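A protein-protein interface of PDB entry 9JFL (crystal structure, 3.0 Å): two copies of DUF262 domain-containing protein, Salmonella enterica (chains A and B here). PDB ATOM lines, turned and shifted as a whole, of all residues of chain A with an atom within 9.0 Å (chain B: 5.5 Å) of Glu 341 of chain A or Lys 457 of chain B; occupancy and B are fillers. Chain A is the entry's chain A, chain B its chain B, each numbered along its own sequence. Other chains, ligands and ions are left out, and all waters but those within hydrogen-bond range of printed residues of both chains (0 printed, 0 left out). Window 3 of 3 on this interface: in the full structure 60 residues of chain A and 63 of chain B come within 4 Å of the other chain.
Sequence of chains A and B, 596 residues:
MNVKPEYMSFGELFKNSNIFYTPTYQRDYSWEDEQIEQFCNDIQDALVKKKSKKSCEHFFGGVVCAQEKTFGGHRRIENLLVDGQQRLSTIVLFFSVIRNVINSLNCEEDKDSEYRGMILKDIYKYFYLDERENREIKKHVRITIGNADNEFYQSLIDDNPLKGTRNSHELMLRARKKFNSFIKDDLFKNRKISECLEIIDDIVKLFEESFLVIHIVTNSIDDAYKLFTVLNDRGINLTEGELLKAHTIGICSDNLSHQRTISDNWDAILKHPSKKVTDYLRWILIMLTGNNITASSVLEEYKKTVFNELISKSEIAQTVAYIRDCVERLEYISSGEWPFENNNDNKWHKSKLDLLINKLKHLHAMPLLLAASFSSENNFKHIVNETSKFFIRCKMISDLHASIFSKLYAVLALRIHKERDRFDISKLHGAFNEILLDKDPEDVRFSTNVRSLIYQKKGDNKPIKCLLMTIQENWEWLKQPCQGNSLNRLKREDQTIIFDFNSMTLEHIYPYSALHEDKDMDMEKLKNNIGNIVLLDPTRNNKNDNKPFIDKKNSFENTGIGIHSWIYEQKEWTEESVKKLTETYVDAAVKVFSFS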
ATOM      1  N   TYR A 332      -2.053   6.680   9.131  1.00  0.00           N
ATOM      2  CA  TYR A 332      -2.579   5.316   9.381  1.00  0.00           C
ATOM      3  C   TYR A 332      -3.945   5.131   8.727  1.00  0.00           C
ATOM      4  O   TYR A 332      -4.147   4.284   7.852  1.00  0.00           O
ATOM      5  CB  TYR A 332      -2.731   5.059  10.885  1.00  0.00           C
ATOM      6  CG  TYR A 332      -1.440   5.031  11.672  1.00  0.00           C
ATOM      7  CD1 TYR A 332      -0.580   3.945  11.594  1.00  0.00           C
ATOM      8  CD2 TYR A 332      -1.096   6.080  12.526  1.00  0.00           C
ATOM      9  CE1 TYR A 332       0.596   3.914  12.325  1.00  0.00           C
ATOM     10  CE2 TYR A 332       0.079   6.056  13.263  1.00  0.00           C
ATOM     11  CZ  TYR A 332       0.923   4.972  13.160  1.00  0.00           C
ATOM     12  OH  TYR A 332       2.091   4.941  13.891  1.00  0.00           O
ATOM     13  N   TRP A 338      -5.145   0.828  11.700  1.00  0.00           N
ATOM     14  CA  TRP A 338      -5.717   1.287  12.953  1.00  0.00           C
ATOM     15  C   TRP A 338      -4.803   2.367  13.551  1.00  0.00           C
ATOM     16  O   TRP A 338      -3.587   2.207  13.547  1.00  0.00           O
ATOM     17  CB  TRP A 338      -5.860   0.078  13.897  1.00  0.00           C
ATOM     18  CG  TRP A 338      -6.926   0.234  14.936  1.00  0.00           C
ATOM     19  CD1 TRP A 338      -6.742   0.428  16.268  1.00  0.00           C
ATOM     20  CD2 TRP A 338      -8.344   0.217  14.723  1.00  0.00           C
ATOM     21  NE1 TRP A 338      -7.959   0.538  16.903  1.00  0.00           N
ATOM     22  CE2 TRP A 338      -8.956   0.412  15.975  1.00  0.00           C
ATOM     23  CE3 TRP A 338      -9.152   0.058  13.596  1.00  0.00           C
ATOM     24  CZ2 TRP A 338     -10.339   0.453  16.132  1.00  0.00           C
ATOM     25  CZ3 TRP A 338     -10.531   0.099  13.757  1.00  0.00           C
ATOM     26  CH2 TRP A 338     -11.108   0.293  15.013  1.00  0.00           C
ATOM     27  N   PRO A 339      -5.375   3.485  14.024  1.00  0.00           N
ATOM     28  CA  PRO A 339      -4.562   4.560  14.629  1.00  0.00           C
ATOM     29  C   PRO A 339      -4.217   4.376  16.113  1.00  0.00           C
ATOM     30  O   PRO A 339      -3.165   4.831  16.550  1.00  0.00           O
ATOM     31  CB  PRO A 339      -5.442   5.804  14.455  1.00  0.00           C
ATOM     32  CG  PRO A 339      -6.829   5.272  14.463  1.00  0.00           C
ATOM     33  CD  PRO A 339      -6.757   3.926  13.781  1.00  0.00           C
ATOM     34  N   PHE A 340      -5.087   3.727  16.879  1.00  0.00           N
ATOM     35  CA  PHE A 340      -4.855   3.547  18.311  1.00  0.00           C
ATOM     36  C   PHE A 340      -3.796   2.482  18.585  1.00  0.00           C
ATOM     37  O   PHE A 340      -3.441   1.700  17.684  1.00  0.00           O
ATOM     38  CB  PHE A 340      -6.157   3.172  19.019  1.00  0.00           C
ATOM     39  CG  PHE A 340      -7.179   4.260  19.004  1.00  0.00           C
ATOM     40  CD1 PHE A 340      -8.067   4.376  17.950  1.00  0.00           C
ATOM     41  CD2 PHE A 340      -7.239   5.182  20.027  1.00  0.00           C
ATOM     42  CE1 PHE A 340      -9.011   5.391  17.923  1.00  0.00           C
ATOM     43  CE2 PHE A 340      -8.177   6.194  20.013  1.00  0.00           C
ATOM     44  CZ  PHE A 340      -9.071   6.300  18.961  1.00  0.00           C
ATOM     45  N   GLU A 341      -3.278   2.485  19.824  1.00  0.00           N
ATOM     46  CA  GLU A 341      -2.429   1.403  20.339  1.00  0.00           C
ATOM     47  C   GLU A 341      -3.169   0.094  20.093  1.00  0.00           C
ATOM     48  O   GLU A 341      -4.227  -0.152  20.682  1.00  0.00           O
ATOM     49  CB  GLU A 341      -2.162   1.577  21.843  1.00  0.00           C
ATOM     50  CG  GLU A 341      -0.964   2.452  22.205  1.00  0.00           C
ATOM     51  CD  GLU A 341       0.354   1.689  22.274  1.00  0.00           C
ATOM     52  OE1 GLU A 341       0.368   0.510  22.695  1.00  0.00           O
ATOM     53  OE2 GLU A 341       1.392   2.286  21.916  1.00  0.00           O
ATOM     54  N   ASN A 342      -2.629  -0.741  19.212  1.00  0.00           N
ATOM     55  CA  ASN A 342      -3.357  -1.930  18.757  1.00  0.00           C
ATOM     56  C   ASN A 342      -3.325  -3.113  19.738  1.00  0.00           C
ATOM     57  O   ASN A 342      -3.832  -4.194  19.427  1.00  0.00           O
ATOM     58  CB  ASN A 342      -2.879  -2.352  17.359  1.00  0.00           C
ATOM     59  CG  ASN A 342      -1.433  -2.806  17.338  1.00  0.00           C
ATOM     60  OD1 ASN A 342      -0.885  -3.241  18.352  1.00  0.00           O
ATOM     61  ND2 ASN A 342      -0.805  -2.705  16.175  1.00  0.00           N
ATOM     62  N   ASN A 343      -2.719  -2.906  20.908  1.00  0.00           N
ATOM     63  CA  ASN A 343      -2.747  -3.899  21.991  1.00  0.00           C
ATOM     64  C   ASN A 343      -4.150  -4.489  22.230  1.00  0.00           C
ATOM     65  O   ASN A 343      -4.346  -5.707  22.092  1.00  0.00           O
ATOM     66  CB  ASN A 343      -2.092  -3.347  23.292  1.00  0.00           C
ATOM     67  CG  ASN A 343      -2.961  -2.341  24.059  1.00  0.00           C
ATOM     68  OD1 ASN A 343      -3.254  -2.543  25.239  1.00  0.00           O
ATOM     69  ND2 ASN A 343      -3.345  -1.248  23.413  1.00  0.00           N
ATOM     70  N   ASN A 344      -5.121  -3.625  22.528  1.00  0.00           N
ATOM     71  CA  ASN A 344      -6.503  -4.044  22.730  1.00  0.00           C
ATOM     72  C   ASN A 344      -7.024  -4.533  21.385  1.00  0.00           C
ATOM     73  O   ASN A 344      -7.408  -3.726  20.531  1.00  0.00           O
ATOM     74  CB  ASN A 344      -7.336  -2.874  23.289  1.00  0.00           C
ATOM     75  CG  ASN A 344      -8.830  -3.179  23.386  1.00  0.00           C
ATOM     76  OD1 ASN A 344      -9.654  -2.271  23.261  1.00  0.00           O
ATOM     77  ND2 ASN A 344      -9.188  -4.443  23.620  1.00  0.00           N
ATOM     78  N   ASP A 345      -7.011  -5.856  21.203  1.00  0.00           N
ATOM     79  CA  ASP A 345      -7.137  -6.463  19.876  1.00  0.00           C
ATOM     80  C   ASP A 345      -8.079  -5.704  18.940  1.00  0.00           C
ATOM     81  O   ASP A 345      -7.620  -5.080  17.982  1.00  0.00           O
ATOM     82  CB  ASP A 345      -7.534  -7.941  19.982  1.00  0.00           C
ATOM     83  CG  ASP A 345      -6.351  -8.837  20.314  1.00  0.00           C
ATOM     84  OD1 ASP A 345      -5.285  -8.716  19.663  1.00  0.00           O
ATOM     85  OD2 ASP A 345      -6.488  -9.667  21.229  1.00  0.00           O
ATOM     86  N   ASN A 346      -9.378  -5.732  19.225  1.00  0.00           N
ATOM     87  CA  ASN A 346     -10.357  -5.067  18.371  1.00  0.00           C
ATOM     88  C   ASN A 346     -10.166  -5.366  16.871  1.00  0.00           C
ATOM     89  O   ASN A 346     -10.297  -4.498  16.020  1.00  0.00           O
ATOM     90  CB  ASN A 346     -10.335  -3.558  18.644  1.00  0.00           C
ATOM     91  CG  ASN A 346     -11.187  -3.164  19.837  1.00  0.00           C
ATOM     92  OD1 ASN A 346     -10.795  -2.311  20.635  1.00  0.00           O
ATOM     93  ND2 ASN A 346     -12.366  -3.771  19.960  1.00  0.00           N
ATOM     94  N   LYS A 350     -10.919  -3.307  13.192  1.00  0.00           N
ATOM     95  CA  LYS A 350      -9.765  -3.185  12.299  1.00  0.00           C
ATOM     96  C   LYS A 350     -10.124  -3.653  10.894  1.00  0.00           C
ATOM     97  O   LYS A 350      -9.779  -3.002   9.923  1.00  0.00           O
ATOM     98  CB  LYS A 350      -8.560  -4.010  12.789  1.00  0.00           C
ATOM     99  CG  LYS A 350      -7.474  -3.221  13.505  1.00  0.00           C
ATOM    100  CD  LYS A 350      -7.676  -3.153  15.021  1.00  0.00           C
ATOM    101  CE  LYS A 350      -6.350  -3.059  15.779  1.00  0.00           C
ATOM    102  NZ  LYS A 350      -5.586  -4.337  15.673  1.00  0.00           N
ATOM    103  N   GLU A 377     -11.887   5.476  21.468  1.00  0.00           N
ATOM    104  CA  GLU A 377     -11.663   4.393  20.513  1.00  0.00           C
ATOM    105  C   GLU A 377     -12.972   3.601  20.310  1.00  0.00           C
ATOM    106  O   GLU A 377     -13.121   2.908  19.310  1.00  0.00           O
ATOM    107  CB  GLU A 377     -10.507   3.486  20.960  1.00  0.00           C
ATOM    108  CG  GLU A 377     -10.380   2.190  20.166  1.00  0.00           C
ATOM    109  CD  GLU A 377      -9.146   1.369  20.500  1.00  0.00           C
ATOM    110  OE1 GLU A 377      -8.380   1.764  21.393  1.00  0.00           O
ATOM    111  OE2 GLU A 377      -8.948   0.310  19.866  1.00  0.00           O
ATOM    112  N   TYR B 455       8.447  -4.952  15.644  1.00  0.00           N
ATOM    113  CA  TYR B 455       6.975  -4.909  15.725  1.00  0.00           C
ATOM    114  C   TYR B 455       6.510  -3.478  16.037  1.00  0.00           C
ATOM    115  O   TYR B 455       7.164  -2.760  16.798  1.00  0.00           O
ATOM    116  CB  TYR B 455       6.453  -5.914  16.782  1.00  0.00           C
ATOM    117  CG  TYR B 455       5.028  -5.699  17.276  1.00  0.00           C
ATOM    118  CD1 TYR B 455       4.750  -4.744  18.252  1.00  0.00           C
ATOM    119  CD2 TYR B 455       3.960  -6.468  16.782  1.00  0.00           C
ATOM    120  CE1 TYR B 455       3.454  -4.544  18.710  1.00  0.00           C
ATOM    121  CE2 TYR B 455       2.661  -6.276  17.236  1.00  0.00           C
ATOM    122  CZ  TYR B 455       2.415  -5.319  18.203  1.00  0.00           C
ATOM    123  OH  TYR B 455       1.139  -5.104  18.678  1.00  0.00           O
ATOM    124  N   GLN B 456       5.393  -3.080  15.419  1.00  0.00           N
ATOM    125  CA  GLN B 456       4.796  -1.753  15.595  1.00  0.00           C
ATOM    126  C   GLN B 456       3.549  -1.769  16.479  1.00  0.00           C
ATOM    127  O   GLN B 456       2.660  -2.604  16.306  1.00  0.00           O
ATOM    128  CB  GLN B 456       4.476  -1.140  14.221  1.00  0.00           C
ATOM    129  CG  GLN B 456       5.715  -0.702  13.444  1.00  0.00           C
ATOM    130  CD  GLN B 456       6.653   0.171  14.280  1.00  0.00           C
ATOM    131  OE1 GLN B 456       6.215   1.083  14.992  1.00  0.00           O
ATOM    132  NE2 GLN B 456       7.948  -0.122  14.213  1.00  0.00           N
ATOM    133  N   LYS B 457       3.484  -0.825  17.413  1.00  0.00           N
ATOM    134  CA  LYS B 457       2.353  -0.724  18.348  1.00  0.00           C
ATOM    135  C   LYS B 457       1.045  -0.156  17.776  1.00  0.00           C
ATOM    136  O   LYS B 457       0.001  -0.260  18.425  1.00  0.00           O
ATOM    137  CB  LYS B 457       2.756   0.092  19.590  1.00  0.00           C
ATOM    138  CG  LYS B 457       3.407   1.446  19.317  1.00  0.00           C
ATOM    139  CD  LYS B 457       4.237   1.916  20.503  1.00  0.00           C
ATOM    140  CE  LYS B 457       5.493   1.078  20.705  1.00  0.00           C
ATOM    141  NZ  LYS B 457       6.366   1.668  21.760  1.00  0.00           N
ATOM    142  N   LYS B 458       1.098   0.461  16.593  1.00  0.00           N
ATOM    143  CA  LYS B 458      -0.079   1.115  16.007  1.00  0.00           C
ATOM    144  C   LYS B 458      -0.495   0.555  14.642  1.00  0.00           C
ATOM    145  O   LYS B 458      -1.691   0.547  14.306  1.00  0.00           O
ATOM    146  CB  LYS B 458       0.159   2.625  15.919  1.00  0.00           C
ATOM    147  CG  LYS B 458      -0.090   3.351  17.233  1.00  0.00           C
ATOM    148  CD  LYS B 458       0.055   4.857  17.094  1.00  0.00           C
ATOM    149  CE  LYS B 458       0.320   5.533  18.435  1.00  0.00           C
ATOM    150  NZ  LYS B 458      -0.829   5.453  19.376  1.00  0.00           N
ATOM    151  N   GLY B 459       0.474   0.059  13.872  1.00  0.00           N
ATOM    152  CA  GLY B 459       0.205  -0.466  12.522  1.00  0.00           C
ATOM    153  C   GLY B 459      -0.808  -1.606  12.382  1.00  0.00           C
ATOM    154  O   GLY B 459      -1.400  -2.056  13.359  1.00  0.00           O
ATOM    155  N   ASN B 461       0.813  -3.660  10.639  1.00  0.00           N
ATOM    156  CA  ASN B 461       2.056  -4.411  10.607  1.00  0.00           C
ATOM    157  C   ASN B 461       2.326  -5.141   9.312  1.00  0.00           C
ATOM    158  O   ASN B 461       2.806  -6.278   9.314  1.00  0.00           O
ATOM    159  CB  ASN B 461       2.117  -5.377  11.782  1.00  0.00           C
ATOM    160  CG  ASN B 461       3.142  -4.961  12.786  1.00  0.00           C
ATOM    161  OD1 ASN B 461       4.337  -4.901  12.465  1.00  0.00           O
ATOM    162  ND2 ASN B 461       2.690  -4.644  14.009  1.00  0.00           N
ATOM    163  N   TYR B 512       4.177  -9.422  25.144  1.00  0.00           N
ATOM    164  CA  TYR B 512       4.116  -8.001  24.842  1.00  0.00           C
ATOM    165  C   TYR B 512       4.040  -7.198  26.137  1.00  0.00           C
ATOM    166  O   TYR B 512       4.869  -6.331  26.373  1.00  0.00           O
ATOM    167  CB  TYR B 512       2.906  -7.684  23.940  1.00  0.00           C
ATOM    168  CG  TYR B 512       2.802  -6.220  23.558  1.00  0.00           C
ATOM    169  CD1 TYR B 512       3.786  -5.613  22.772  1.00  0.00           C
ATOM    170  CD2 TYR B 512       1.740  -5.434  23.990  1.00  0.00           C
ATOM    171  CE1 TYR B 512       3.713  -4.266  22.425  1.00  0.00           C
ATOM    172  CE2 TYR B 512       1.659  -4.083  23.649  1.00  0.00           C
ATOM    173  CZ  TYR B 512       2.649  -3.503  22.865  1.00  0.00           C
ATOM    174  OH  TYR B 512       2.581  -2.170  22.514  1.00  0.00           O
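O of Lys 458 of chain B lies close to O of Trp 338 of chain A, 2.6 Å away. OH of Tyr 512 of chain B lies within hydrogen-bond range of OE1 of Glu 341 of chain A, 3.5 Å away. ND2 of Asn 342 of chain A sits at hydrogen-bond distance from O of Gly 459 of chain B (3.0 Å). The backbone carbonyl oxygen of Gln 456 of chain B sits at hydrogen-bond distance from the side-chain amide nitrogen of Asn 342 of chain A (3.5 Å). The backbone carbonyl oxygen of Lys 457 of chain B sits at hydrogen-bond distance from the backbone NH of Asn 342 of chain A, 2.8 Å away. OH of Tyr 455 of chain B lies within hydrogen-bond range of OD1 of Asn 342 of chain A (2.8 Å).
No position is printed for both chains. Of the 13 pairs that touch across the chains among the printed residues, none has its exchanged pair printed and touching as well.
The indole nitrogen (NE1) of Trp 338 of chain A sits at hydrogen-bond distance from the side-chain carboxylate (OE2) of Glu 377 of chain A (3.1 Å). O of Gln 456 of chain B lies within hydrogen-bond range of ND2 of Asn 461 of chain B (3.1 Å). The backbone carbonyl oxygen (O) of Glu 341 of chain A sits at hydrogen-bond distance from the side-chain amide nitrogen (ND2) of Asn 343 of chain A (3.1 Å).
Of the printed residues of chain B, Tyr 332 of chain A touches Lys 458 (3.6 Å). Of the printed residues of chain B, Trp 338 of chain A touches Lys 458. Glu 341 of chain A touches just these residues of chain B: Lys 457 (3.2 Å), Lys 458 (3.9 Å) and Tyr 512 (3.5 Å). Asp 345 of chain A touches none of the printed residues of chain B. Of the printed residues of chain A, Tyr 455 of chain B touches Asn 342. Of chain A, only Glu 341 and Asn 342 come within 4 Å of Lys 457 of chain B. Of chain A, only Tyr 332, Trp 338, Pro 339, Phe 340, Glu 341 and Asn 342 come within 4 Å of Lys 458 of chain B. Of the printed residues of chain A, Gly 459 of chain B touches Asn 342 (3.0 Å). Printed residues of chain A within 4 Å of Tyr 512 of chain B: Glu 341 (3.5 Å) and Asn 343 (3.8 Å). The nearest printed residue of chain A that does not touch Gly 459 of chain B is Tyr 332 of chain A (4.2 Å).
Of the 7 printed residues of chain B, 6 touch a printed residue of chain A. Printed residues of chain B that touch a printed residue of chain A: Tyr 455, Gln 456, Lys 457, Lys 458, Gly 459 and Tyr 512. Hydrophobic or aromatic side chains of chain B within 4 Å of the printed part of chain A: Tyr 455 and Tyr 512. Hydrophobic or aromatic side chains of chain A within 4 Å of the printed part of chain B: Tyr 332.
Among the printed residues, pairs that only touch across the chains: Glu 341 of chain A with Lys 457 of chain B (3.2 Å), Pro 339 of chain A with Lys 458 of chain B (3.3 Å), Asn 342 of chain A with Lys 458 of chain B (3.6 Å), Tyr 332 of chain A with Lys 458 of chain B (3.6 Å), Phe 340 of chain A with Lys 458 of chain B (3.8 Å), Asn 343 of chain A with Tyr 512 of chain B (3.8 Å) and Glu 341 of chain A with Lys 458 of chain B (3.9 Å).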
